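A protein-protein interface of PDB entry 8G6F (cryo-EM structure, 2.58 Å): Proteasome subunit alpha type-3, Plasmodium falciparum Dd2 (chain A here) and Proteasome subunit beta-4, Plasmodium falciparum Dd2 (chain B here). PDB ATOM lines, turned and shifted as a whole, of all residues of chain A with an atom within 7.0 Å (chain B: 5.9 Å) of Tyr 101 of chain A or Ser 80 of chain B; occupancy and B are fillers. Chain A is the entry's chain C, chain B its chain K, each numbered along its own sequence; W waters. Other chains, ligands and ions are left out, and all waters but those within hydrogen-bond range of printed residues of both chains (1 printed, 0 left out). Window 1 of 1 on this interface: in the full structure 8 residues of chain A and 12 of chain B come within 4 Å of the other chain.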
ATOM      1  N   ARG A  96      -8.323  35.920   4.351  1.00  0.00           N
ATOM      2  CA  ARG A  96      -7.131  36.301   5.097  1.00  0.00           C
ATOM      3  C   ARG A  96      -6.047  35.242   4.975  1.00  0.00           C
ATOM      4  O   ARG A  96      -4.866  35.567   4.826  1.00  0.00           O
ATOM      5  CB  ARG A  96      -7.494  36.537   6.562  1.00  0.00           C
ATOM      6  CG  ARG A  96      -6.381  37.122   7.404  1.00  0.00           C
ATOM      7  CD  ARG A  96      -6.337  38.627   7.287  1.00  0.00           C
ATOM      8  NE  ARG A  96      -5.031  39.164   7.648  1.00  0.00           N
ATOM      9  CZ  ARG A  96      -4.609  40.381   7.335  1.00  0.00           C
ATOM     10  NH1 ARG A  96      -5.365  41.221   6.649  1.00  0.00           N
ATOM     11  NH2 ARG A  96      -3.395  40.764   7.721  1.00  0.00           N
ATOM     12  N   TYR A  97      -6.425  33.966   5.044  1.00  0.00           N
ATOM     13  CA  TYR A  97      -5.435  32.910   4.859  1.00  0.00           C
ATOM     14  C   TYR A  97      -4.836  32.961   3.463  1.00  0.00           C
ATOM     15  O   TYR A  97      -3.623  32.794   3.294  1.00  0.00           O
ATOM     16  CB  TYR A  97      -6.055  31.540   5.113  1.00  0.00           C
ATOM     17  CG  TYR A  97      -5.060  30.404   5.040  1.00  0.00           C
ATOM     18  CD1 TYR A  97      -4.606  29.925   3.821  1.00  0.00           C
ATOM     19  CD2 TYR A  97      -4.574  29.807   6.192  1.00  0.00           C
ATOM     20  CE1 TYR A  97      -3.697  28.894   3.750  1.00  0.00           C
ATOM     21  CE2 TYR A  97      -3.666  28.770   6.130  1.00  0.00           C
ATOM     22  CZ  TYR A  97      -3.234  28.320   4.908  1.00  0.00           C
ATOM     23  OH  TYR A  97      -2.332  27.290   4.839  1.00  0.00           O
ATOM     24  N   LEU A  98      -5.672  33.155   2.443  1.00  0.00           N
ATOM     25  CA  LEU A  98      -5.135  33.252   1.090  1.00  0.00           C
ATOM     26  C   LEU A  98      -4.192  34.441   0.969  1.00  0.00           C
ATOM     27  O   LEU A  98      -3.138  34.347   0.336  1.00  0.00           O
ATOM     28  CB  LEU A  98      -6.273  33.350   0.075  1.00  0.00           C
ATOM     29  CG  LEU A  98      -5.879  33.575  -1.385  1.00  0.00           C
ATOM     30  CD1 LEU A  98      -4.873  32.550  -1.856  1.00  0.00           C
ATOM     31  CD2 LEU A  98      -7.102  33.548  -2.269  1.00  0.00           C
ATOM     32  N   TYR A  99      -4.545  35.561   1.595  1.00  0.00           N
ATOM     33  CA  TYR A  99      -3.686  36.736   1.583  1.00  0.00           C
ATOM     34  C   TYR A  99      -2.351  36.459   2.266  1.00  0.00           C
ATOM     35  O   TYR A  99      -1.302  36.917   1.804  1.00  0.00           O
ATOM     36  CB  TYR A  99      -4.425  37.889   2.262  1.00  0.00           C
ATOM     37  CG  TYR A  99      -3.612  39.129   2.519  1.00  0.00           C
ATOM     38  CD1 TYR A  99      -3.488  40.111   1.554  1.00  0.00           C
ATOM     39  CD2 TYR A  99      -2.997  39.335   3.743  1.00  0.00           C
ATOM     40  CE1 TYR A  99      -2.756  41.250   1.788  1.00  0.00           C
ATOM     41  CE2 TYR A  99      -2.263  40.472   3.988  1.00  0.00           C
ATOM     42  CZ  TYR A  99      -2.148  41.428   3.008  1.00  0.00           C
ATOM     43  OH  TYR A  99      -1.418  42.567   3.245  1.00  0.00           O
ATOM     44  N   ASN A 100      -2.373  35.709   3.368  1.00  0.00           N
ATOM     45  CA  ASN A 100      -1.163  35.476   4.150  1.00  0.00           C
ATOM     46  C   ASN A 100      -0.241  34.443   3.512  1.00  0.00           C
ATOM     47  O   ASN A 100       0.983  34.579   3.591  1.00  0.00           O
ATOM     48  CB  ASN A 100      -1.530  35.025   5.561  1.00  0.00           C
ATOM     49  CG  ASN A 100      -1.859  36.180   6.475  1.00  0.00           C
ATOM     50  OD1 ASN A 100      -1.281  37.258   6.365  1.00  0.00           O
ATOM     51  ND2 ASN A 100      -2.791  35.959   7.391  1.00  0.00           N
ATOM     52  N   TYR A 101      -0.797  33.404   2.890  1.00  0.00           N
ATOM     53  CA  TYR A 101       0.000  32.261   2.467  1.00  0.00           C
ATOM     54  C   TYR A 101       0.011  32.002   0.969  1.00  0.00           C
ATOM     55  O   TYR A 101       0.722  31.094   0.531  1.00  0.00           O
ATOM     56  CB  TYR A 101      -0.491  30.989   3.172  1.00  0.00           C
ATOM     57  CG  TYR A 101      -0.279  31.014   4.663  1.00  0.00           C
ATOM     58  CD1 TYR A 101       0.942  30.670   5.212  1.00  0.00           C
ATOM     59  CD2 TYR A 101      -1.300  31.386   5.522  1.00  0.00           C
ATOM     60  CE1 TYR A 101       1.139  30.692   6.569  1.00  0.00           C
ATOM     61  CE2 TYR A 101      -1.110  31.413   6.878  1.00  0.00           C
ATOM     62  CZ  TYR A 101       0.111  31.065   7.398  1.00  0.00           C
ATOM     63  OH  TYR A 101       0.305  31.087   8.755  1.00  0.00           O
ATOM     64  N   ASN A 102      -0.737  32.759   0.171  1.00  0.00           N
ATOM     65  CA  ASN A 102      -0.810  32.556  -1.271  1.00  0.00           C
ATOM     66  C   ASN A 102      -1.398  31.202  -1.640  1.00  0.00           C
ATOM     67  O   ASN A 102      -1.210  30.727  -2.762  1.00  0.00           O
ATOM     68  CB  ASN A 102       0.565  32.713  -1.921  1.00  0.00           C
ATOM     69  CG  ASN A 102       0.491  33.352  -3.285  1.00  0.00           C
ATOM     70  OD1 ASN A 102      -0.352  34.202  -3.538  1.00  0.00           O
ATOM     71  ND2 ASN A 102       1.373  32.939  -4.175  1.00  0.00           N
ATOM     72  N   GLU A 103      -2.114  30.565  -0.717  1.00  0.00           N
ATOM     73  CA  GLU A 103      -2.764  29.290  -0.975  1.00  0.00           C
ATOM     74  C   GLU A 103      -4.105  29.280  -0.258  1.00  0.00           C
ATOM     75  O   GLU A 103      -4.341  30.067   0.658  1.00  0.00           O
ATOM     76  CB  GLU A 103      -1.901  28.108  -0.516  1.00  0.00           C
ATOM     77  CG  GLU A 103      -0.501  28.072  -1.124  1.00  0.00           C
ATOM     78  CD  GLU A 103      -0.288  26.914  -2.075  1.00  0.00           C
ATOM     79  OE1 GLU A 103      -1.279  26.377  -2.611  1.00  0.00           O
ATOM     80  OE2 GLU A 103       0.879  26.533  -2.289  1.00  0.00           O
ATOM     81  N   VAL A 104      -4.986  28.385  -0.685  1.00  0.00           N
ATOM     82  CA  VAL A 104      -6.336  28.321  -0.130  1.00  0.00           C
ATOM     83  C   VAL A 104      -6.299  27.639   1.230  1.00  0.00           C
ATOM     84  O   VAL A 104      -5.566  26.667   1.439  1.00  0.00           O
ATOM     85  CB  VAL A 104      -7.289  27.595  -1.095  1.00  0.00           C
ATOM     86  CG1 VAL A 104      -7.384  28.351  -2.404  1.00  0.00           C
ATOM     87  CG2 VAL A 104      -6.855  26.160  -1.325  1.00  0.00           C
ATOM     88  N   GLN A 109      -8.736  24.007   9.083  1.00  0.00           N
ATOM     89  CA  GLN A 109      -8.266  25.255   9.670  1.00  0.00           C
ATOM     90  C   GLN A 109      -9.381  26.290   9.736  1.00  0.00           C
ATOM     91  O   GLN A 109      -9.536  26.988  10.749  1.00  0.00           O
ATOM     92  CB  GLN A 109      -7.084  25.789   8.870  1.00  0.00           C
ATOM     93  CG  GLN A 109      -5.917  24.836   8.822  1.00  0.00           C
ATOM     94  CD  GLN A 109      -4.635  25.508   8.406  1.00  0.00           C
ATOM     95  OE1 GLN A 109      -4.484  26.717   8.547  1.00  0.00           O
ATOM     96  NE2 GLN A 109      -3.699  24.727   7.892  1.00  0.00           N
ATOM     97  N   LYS A 142      -4.903  18.340   0.973  1.00  0.00           N
ATOM     98  CA  LYS A 142      -4.280  17.653   2.097  1.00  0.00           C
ATOM     99  C   LYS A 142      -5.146  16.497   2.586  1.00  0.00           C
ATOM    100  O   LYS A 142      -4.680  15.357   2.667  1.00  0.00           O
ATOM    101  CB  LYS A 142      -4.014  18.639   3.235  1.00  0.00           C
ATOM    102  CG  LYS A 142      -3.117  19.794   2.841  1.00  0.00           C
ATOM    103  CD  LYS A 142      -2.698  20.623   4.040  1.00  0.00           C
ATOM    104  CE  LYS A 142      -1.642  21.645   3.655  1.00  0.00           C
ATOM    105  NZ  LYS A 142      -1.172  22.449   4.815  1.00  0.00           N
ATOM    106  N   TYR B  68       3.022  26.808  13.121  1.00  0.00           N
ATOM    107  CA  TYR B  68       1.967  26.471  12.172  1.00  0.00           C
ATOM    108  C   TYR B  68       1.857  24.963  12.008  1.00  0.00           C
ATOM    109  O   TYR B  68       0.759  24.393  12.061  1.00  0.00           O
ATOM    110  CB  TYR B  68       2.246  27.141  10.826  1.00  0.00           C
ATOM    111  CG  TYR B  68       1.330  26.696   9.708  1.00  0.00           C
ATOM    112  CD1 TYR B  68       1.565  25.517   9.014  1.00  0.00           C
ATOM    113  CD2 TYR B  68       0.233  27.457   9.341  1.00  0.00           C
ATOM    114  CE1 TYR B  68       0.732  25.111   8.003  1.00  0.00           C
ATOM    115  CE2 TYR B  68      -0.603  27.057   8.327  1.00  0.00           C
ATOM    116  CZ  TYR B  68      -0.350  25.885   7.663  1.00  0.00           C
ATOM    117  OH  TYR B  68      -1.183  25.484   6.651  1.00  0.00           O
ATOM    118  N   MET B  76       3.800  22.536   6.136  1.00  0.00           N
ATOM    119  CA  MET B  76       3.531  23.690   5.294  1.00  0.00           C
ATOM    120  C   MET B  76       4.136  23.476   3.913  1.00  0.00           C
ATOM    121  O   MET B  76       5.244  22.952   3.778  1.00  0.00           O
ATOM    122  CB  MET B  76       4.104  24.953   5.935  1.00  0.00           C
ATOM    123  CG  MET B  76       3.456  26.237   5.468  1.00  0.00           C
ATOM    124  SD  MET B  76       4.453  27.696   5.806  1.00  0.00           S
ATOM    125  CE  MET B  76       3.807  28.204   7.388  1.00  0.00           C
ATOM    126  N   PHE B  77       3.396  23.871   2.879  1.00  0.00           N
ATOM    127  CA  PHE B  77       3.914  23.785   1.525  1.00  0.00           C
ATOM    128  C   PHE B  77       5.065  24.766   1.337  1.00  0.00           C
ATOM    129  O   PHE B  77       5.171  25.780   2.028  1.00  0.00           O
ATOM    130  CB  PHE B  77       2.818  24.080   0.503  1.00  0.00           C
ATOM    131  CG  PHE B  77       1.745  23.034   0.439  1.00  0.00           C
ATOM    132  CD1 PHE B  77       2.064  21.692   0.373  1.00  0.00           C
ATOM    133  CD2 PHE B  77       0.410  23.399   0.433  1.00  0.00           C
ATOM    134  CE1 PHE B  77       1.074  20.734   0.311  1.00  0.00           C
ATOM    135  CE2 PHE B  77      -0.582  22.446   0.372  1.00  0.00           C
ATOM    136  CZ  PHE B  77      -0.250  21.112   0.312  1.00  0.00           C
ATOM    137  N   VAL B  78       5.939  24.451   0.382  1.00  0.00           N
ATOM    138  CA  VAL B  78       7.103  25.296   0.141  1.00  0.00           C
ATOM    139  C   VAL B  78       6.676  26.653  -0.403  1.00  0.00           C
ATOM    140  O   VAL B  78       7.260  27.684  -0.059  1.00  0.00           O
ATOM    141  CB  VAL B  78       8.089  24.590  -0.804  1.00  0.00           C
ATOM    142  CG1 VAL B  78       9.355  25.405  -0.954  1.00  0.00           C
ATOM    143  CG2 VAL B  78       8.409  23.205  -0.287  1.00  0.00           C
ATOM    144  N   LYS B  79       5.661  26.679  -1.268  1.00  0.00           N
ATOM    145  CA  LYS B  79       5.172  27.951  -1.786  1.00  0.00           C
ATOM    146  C   LYS B  79       4.552  28.796  -0.681  1.00  0.00           C
ATOM    147  O   LYS B  79       4.794  30.008  -0.604  1.00  0.00           O
ATOM    148  CB  LYS B  79       4.163  27.703  -2.902  1.00  0.00           C
ATOM    149  CG  LYS B  79       3.623  28.970  -3.528  1.00  0.00           C
ATOM    150  CD  LYS B  79       2.863  28.679  -4.802  1.00  0.00           C
ATOM    151  CE  LYS B  79       1.783  29.713  -5.051  1.00  0.00           C
ATOM    152  NZ  LYS B  79       0.881  29.310  -6.158  1.00  0.00           N
ATOM    153  N   SER B  80       3.751  28.173   0.187  1.00  0.00           N
ATOM    154  CA  SER B  80       3.186  28.897   1.318  1.00  0.00           C
ATOM    155  C   SER B  80       4.286  29.443   2.211  1.00  0.00           C
ATOM    156  O   SER B  80       4.211  30.583   2.673  1.00  0.00           O
ATOM    157  CB  SER B  80       2.266  27.985   2.120  1.00  0.00           C
ATOM    158  OG  SER B  80       1.489  27.174   1.267  1.00  0.00           O
ATOM    159  N   PHE B  81       5.316  28.638   2.461  1.00  0.00           N
ATOM    160  CA  PHE B  81       6.430  29.067   3.297  1.00  0.00           C
ATOM    161  C   PHE B  81       7.158  30.255   2.675  1.00  0.00           C
ATOM    162  O   PHE B  81       7.449  31.248   3.354  1.00  0.00           O
ATOM    163  CB  PHE B  81       7.366  27.875   3.502  1.00  0.00           C
ATOM    164  CG  PHE B  81       8.718  28.232   4.024  1.00  0.00           C
ATOM    165  CD1 PHE B  81       8.860  28.967   5.181  1.00  0.00           C
ATOM    166  CD2 PHE B  81       9.853  27.807   3.363  1.00  0.00           C
ATOM    167  CE1 PHE B  81      10.106  29.283   5.659  1.00  0.00           C
ATOM    168  CE2 PHE B  81      11.101  28.122   3.841  1.00  0.00           C
ATOM    169  CZ  PHE B  81      11.228  28.861   4.986  1.00  0.00           C
ATOM    170  N   ALA B  82       7.434  30.182   1.375  1.00  0.00           N
ATOM    171  CA  ALA B  82       8.145  31.261   0.700  1.00  0.00           C
ATOM    172  C   ALA B  82       7.342  32.553   0.731  1.00  0.00           C
ATOM    173  O   ALA B  82       7.880  33.626   1.024  1.00  0.00           O
ATOM    174  CB  ALA B  82       8.456  30.858  -0.739  1.00  0.00           C
ATOM    175  N   PHE B  83       6.047  32.474   0.435  1.00  0.00           N
ATOM    176  CA  PHE B  83       5.254  33.693   0.387  1.00  0.00           C
ATOM    177  C   PHE B  83       4.945  34.228   1.778  1.00  0.00           C
ATOM    178  O   PHE B  83       4.818  35.440   1.950  1.00  0.00           O
ATOM    179  CB  PHE B  83       3.978  33.449  -0.412  1.00  0.00           C
ATOM    180  CG  PHE B  83       4.183  33.557  -1.890  1.00  0.00           C
ATOM    181  CD1 PHE B  83       4.138  34.785  -2.519  1.00  0.00           C
ATOM    182  CD2 PHE B  83       4.454  32.435  -2.646  1.00  0.00           C
ATOM    183  CE1 PHE B  83       4.339  34.887  -3.871  1.00  0.00           C
ATOM    184  CE2 PHE B  83       4.659  32.533  -3.998  1.00  0.00           C
ATOM    185  CZ  PHE B  83       4.601  33.759  -4.614  1.00  0.00           C
ATOM    186  N   PHE B  84       4.861  33.358   2.783  1.00  0.00           N
ATOM    187  CA  PHE B  84       4.773  33.816   4.163  1.00  0.00           C
ATOM    188  C   PHE B  84       6.026  34.586   4.563  1.00  0.00           C
ATOM    189  O   PHE B  84       5.941  35.660   5.174  1.00  0.00           O
ATOM    190  CB  PHE B  84       4.552  32.601   5.069  1.00  0.00           C
ATOM    191  CG  PHE B  84       4.525  32.918   6.530  1.00  0.00           C
ATOM    192  CD1 PHE B  84       3.396  33.452   7.116  1.00  0.00           C
ATOM    193  CD2 PHE B  84       5.623  32.659   7.323  1.00  0.00           C
ATOM    194  CE1 PHE B  84       3.372  33.735   8.459  1.00  0.00           C
ATOM    195  CE2 PHE B  84       5.603  32.942   8.664  1.00  0.00           C
ATOM    196  CZ  PHE B  84       4.477  33.480   9.233  1.00  0.00           C
ATOM    197  N   THR B  85       7.199  34.059   4.210  1.00  0.00           N
ATOM    198  CA  THR B  85       8.447  34.759   4.495  1.00  0.00           C
ATOM    199  C   THR B  85       8.485  36.111   3.796  1.00  0.00           C
ATOM    200  O   THR B  85       8.863  37.127   4.394  1.00  0.00           O
ATOM    201  CB  THR B  85       9.632  33.902   4.053  1.00  0.00           C
ATOM    202  OG1 THR B  85       9.491  32.579   4.577  1.00  0.00           O
ATOM    203  CG2 THR B  85      10.937  34.499   4.530  1.00  0.00           C
ATOM    204  N   LYS B 110       3.214  18.319  -3.958  1.00  0.00           N
ATOM    205  CA  LYS B 110       2.365  19.093  -4.856  1.00  0.00           C
ATOM    206  C   LYS B 110       3.179  19.733  -5.973  1.00  0.00           C
ATOM    207  O   LYS B 110       2.791  19.678  -7.145  1.00  0.00           O
ATOM    208  CB  LYS B 110       1.615  20.162  -4.063  1.00  0.00           C
ATOM    209  CG  LYS B 110       0.696  21.041  -4.904  1.00  0.00           C
ATOM    210  CD  LYS B 110       0.183  22.242  -4.124  1.00  0.00           C
ATOM    211  CE  LYS B 110       1.322  23.115  -3.618  1.00  0.00           C
ATOM    212  NZ  LYS B 110       0.879  24.503  -3.329  1.00  0.00           N
HETATM  213  O   HOH W   1       0.706  24.299   3.653  1.00  0.00           O
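Hydrophobic or aromatic side chains of chain B that line the printed part of chain A: Tyr 68, Met 76, Phe 77, Phe 83 and Phe 84.
Along chain B the printed residues that touch a printed residue of chain A span positions 68 to 110.
Hydrophobic or aromatic side chains of chain A that line the printed part of chain B: Tyr 97 and Tyr 101.
Tyr 101 of chain A touches four residues of chain B.
Of the printed residues of chain A, Lys 110 of chain B touches Glu 103 (2.3 Å).
Of the printed residues of chain B, Glu 103 of chain A touches Lys 79 (3.5 Å), Ser 80 (3.2 Å) and Lys 110 (2.3 Å).
Phe 81 of chain B touches none of the printed residues of chain A.
Leu 98 of chain A touches none of the printed residues of chain B.
The nearest residue of chain B that does not touch Tyr 101 of chain A is Phe 83 of chain B (4.1 Å).
The nearest printed residue of chain A that does not touch Ser 80 of chain B is Asn 100 of chain A (5.2 Å).
The nearest printed residue of chain A that does not touch Lys 110 of chain B is Asn 102 of chain A (6.6 Å).
SD of Met 76 of chain B sits close to N of Phe 81 of chain B, at 3.6 Å.
The backbone carbonyl oxygen of Arg 96 of chain A lies within hydrogen-bond range of the side-chain amide nitrogen of Asn 100 of chain A (3.3 Å).
Water W1 bridges the backbone NH (N) of Phe 77 of chain B (2.8 Å) and the side-chain amino group (NZ) of Lys 142 of chain A (2.9 Å).
OH of Tyr 68 of chain B lies within hydrogen-bond range of OH of Tyr 97 of chain A (2.8 Å).
NE2 of Gln 109 of chain A sits at hydrogen-bond distance from OH of Tyr 68 of chain B.
NZ of Lys 110 of chain B is in salt-bridge range of OE1 of Glu 103 of chain A (2.9 Å).
Among the printed residues, merely in contact across the chains: Asn 100 of chain A with Phe 84 of chain B (3.9 Å), Tyr 101 of chain A with Tyr 68 of chain B (3.7 Å), Tyr 101 of chain A with Met 76 of chain B (3.7 Å), Tyr 101 of chain A with Ser 80 of chain B (3.4 Å), Tyr 101 of chain A with Phe 84 of chain B (3.6 Å), Asn 102 of chain A with Lys 79 of chain B (3.4 Å), Asn 102 of chain A with Phe 83 of chain B (3.3 Å), Glu 103 of chain A with Lys 79 of chain B (3.5 Å), Glu 103 of chain A with Ser 80 of chain B (3.2 Å), Lys 142 of chain A with Tyr 68 of chain B (3.5 Å) and Lys 142 of chain A with Phe 77 of chain B (3.5 Å).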
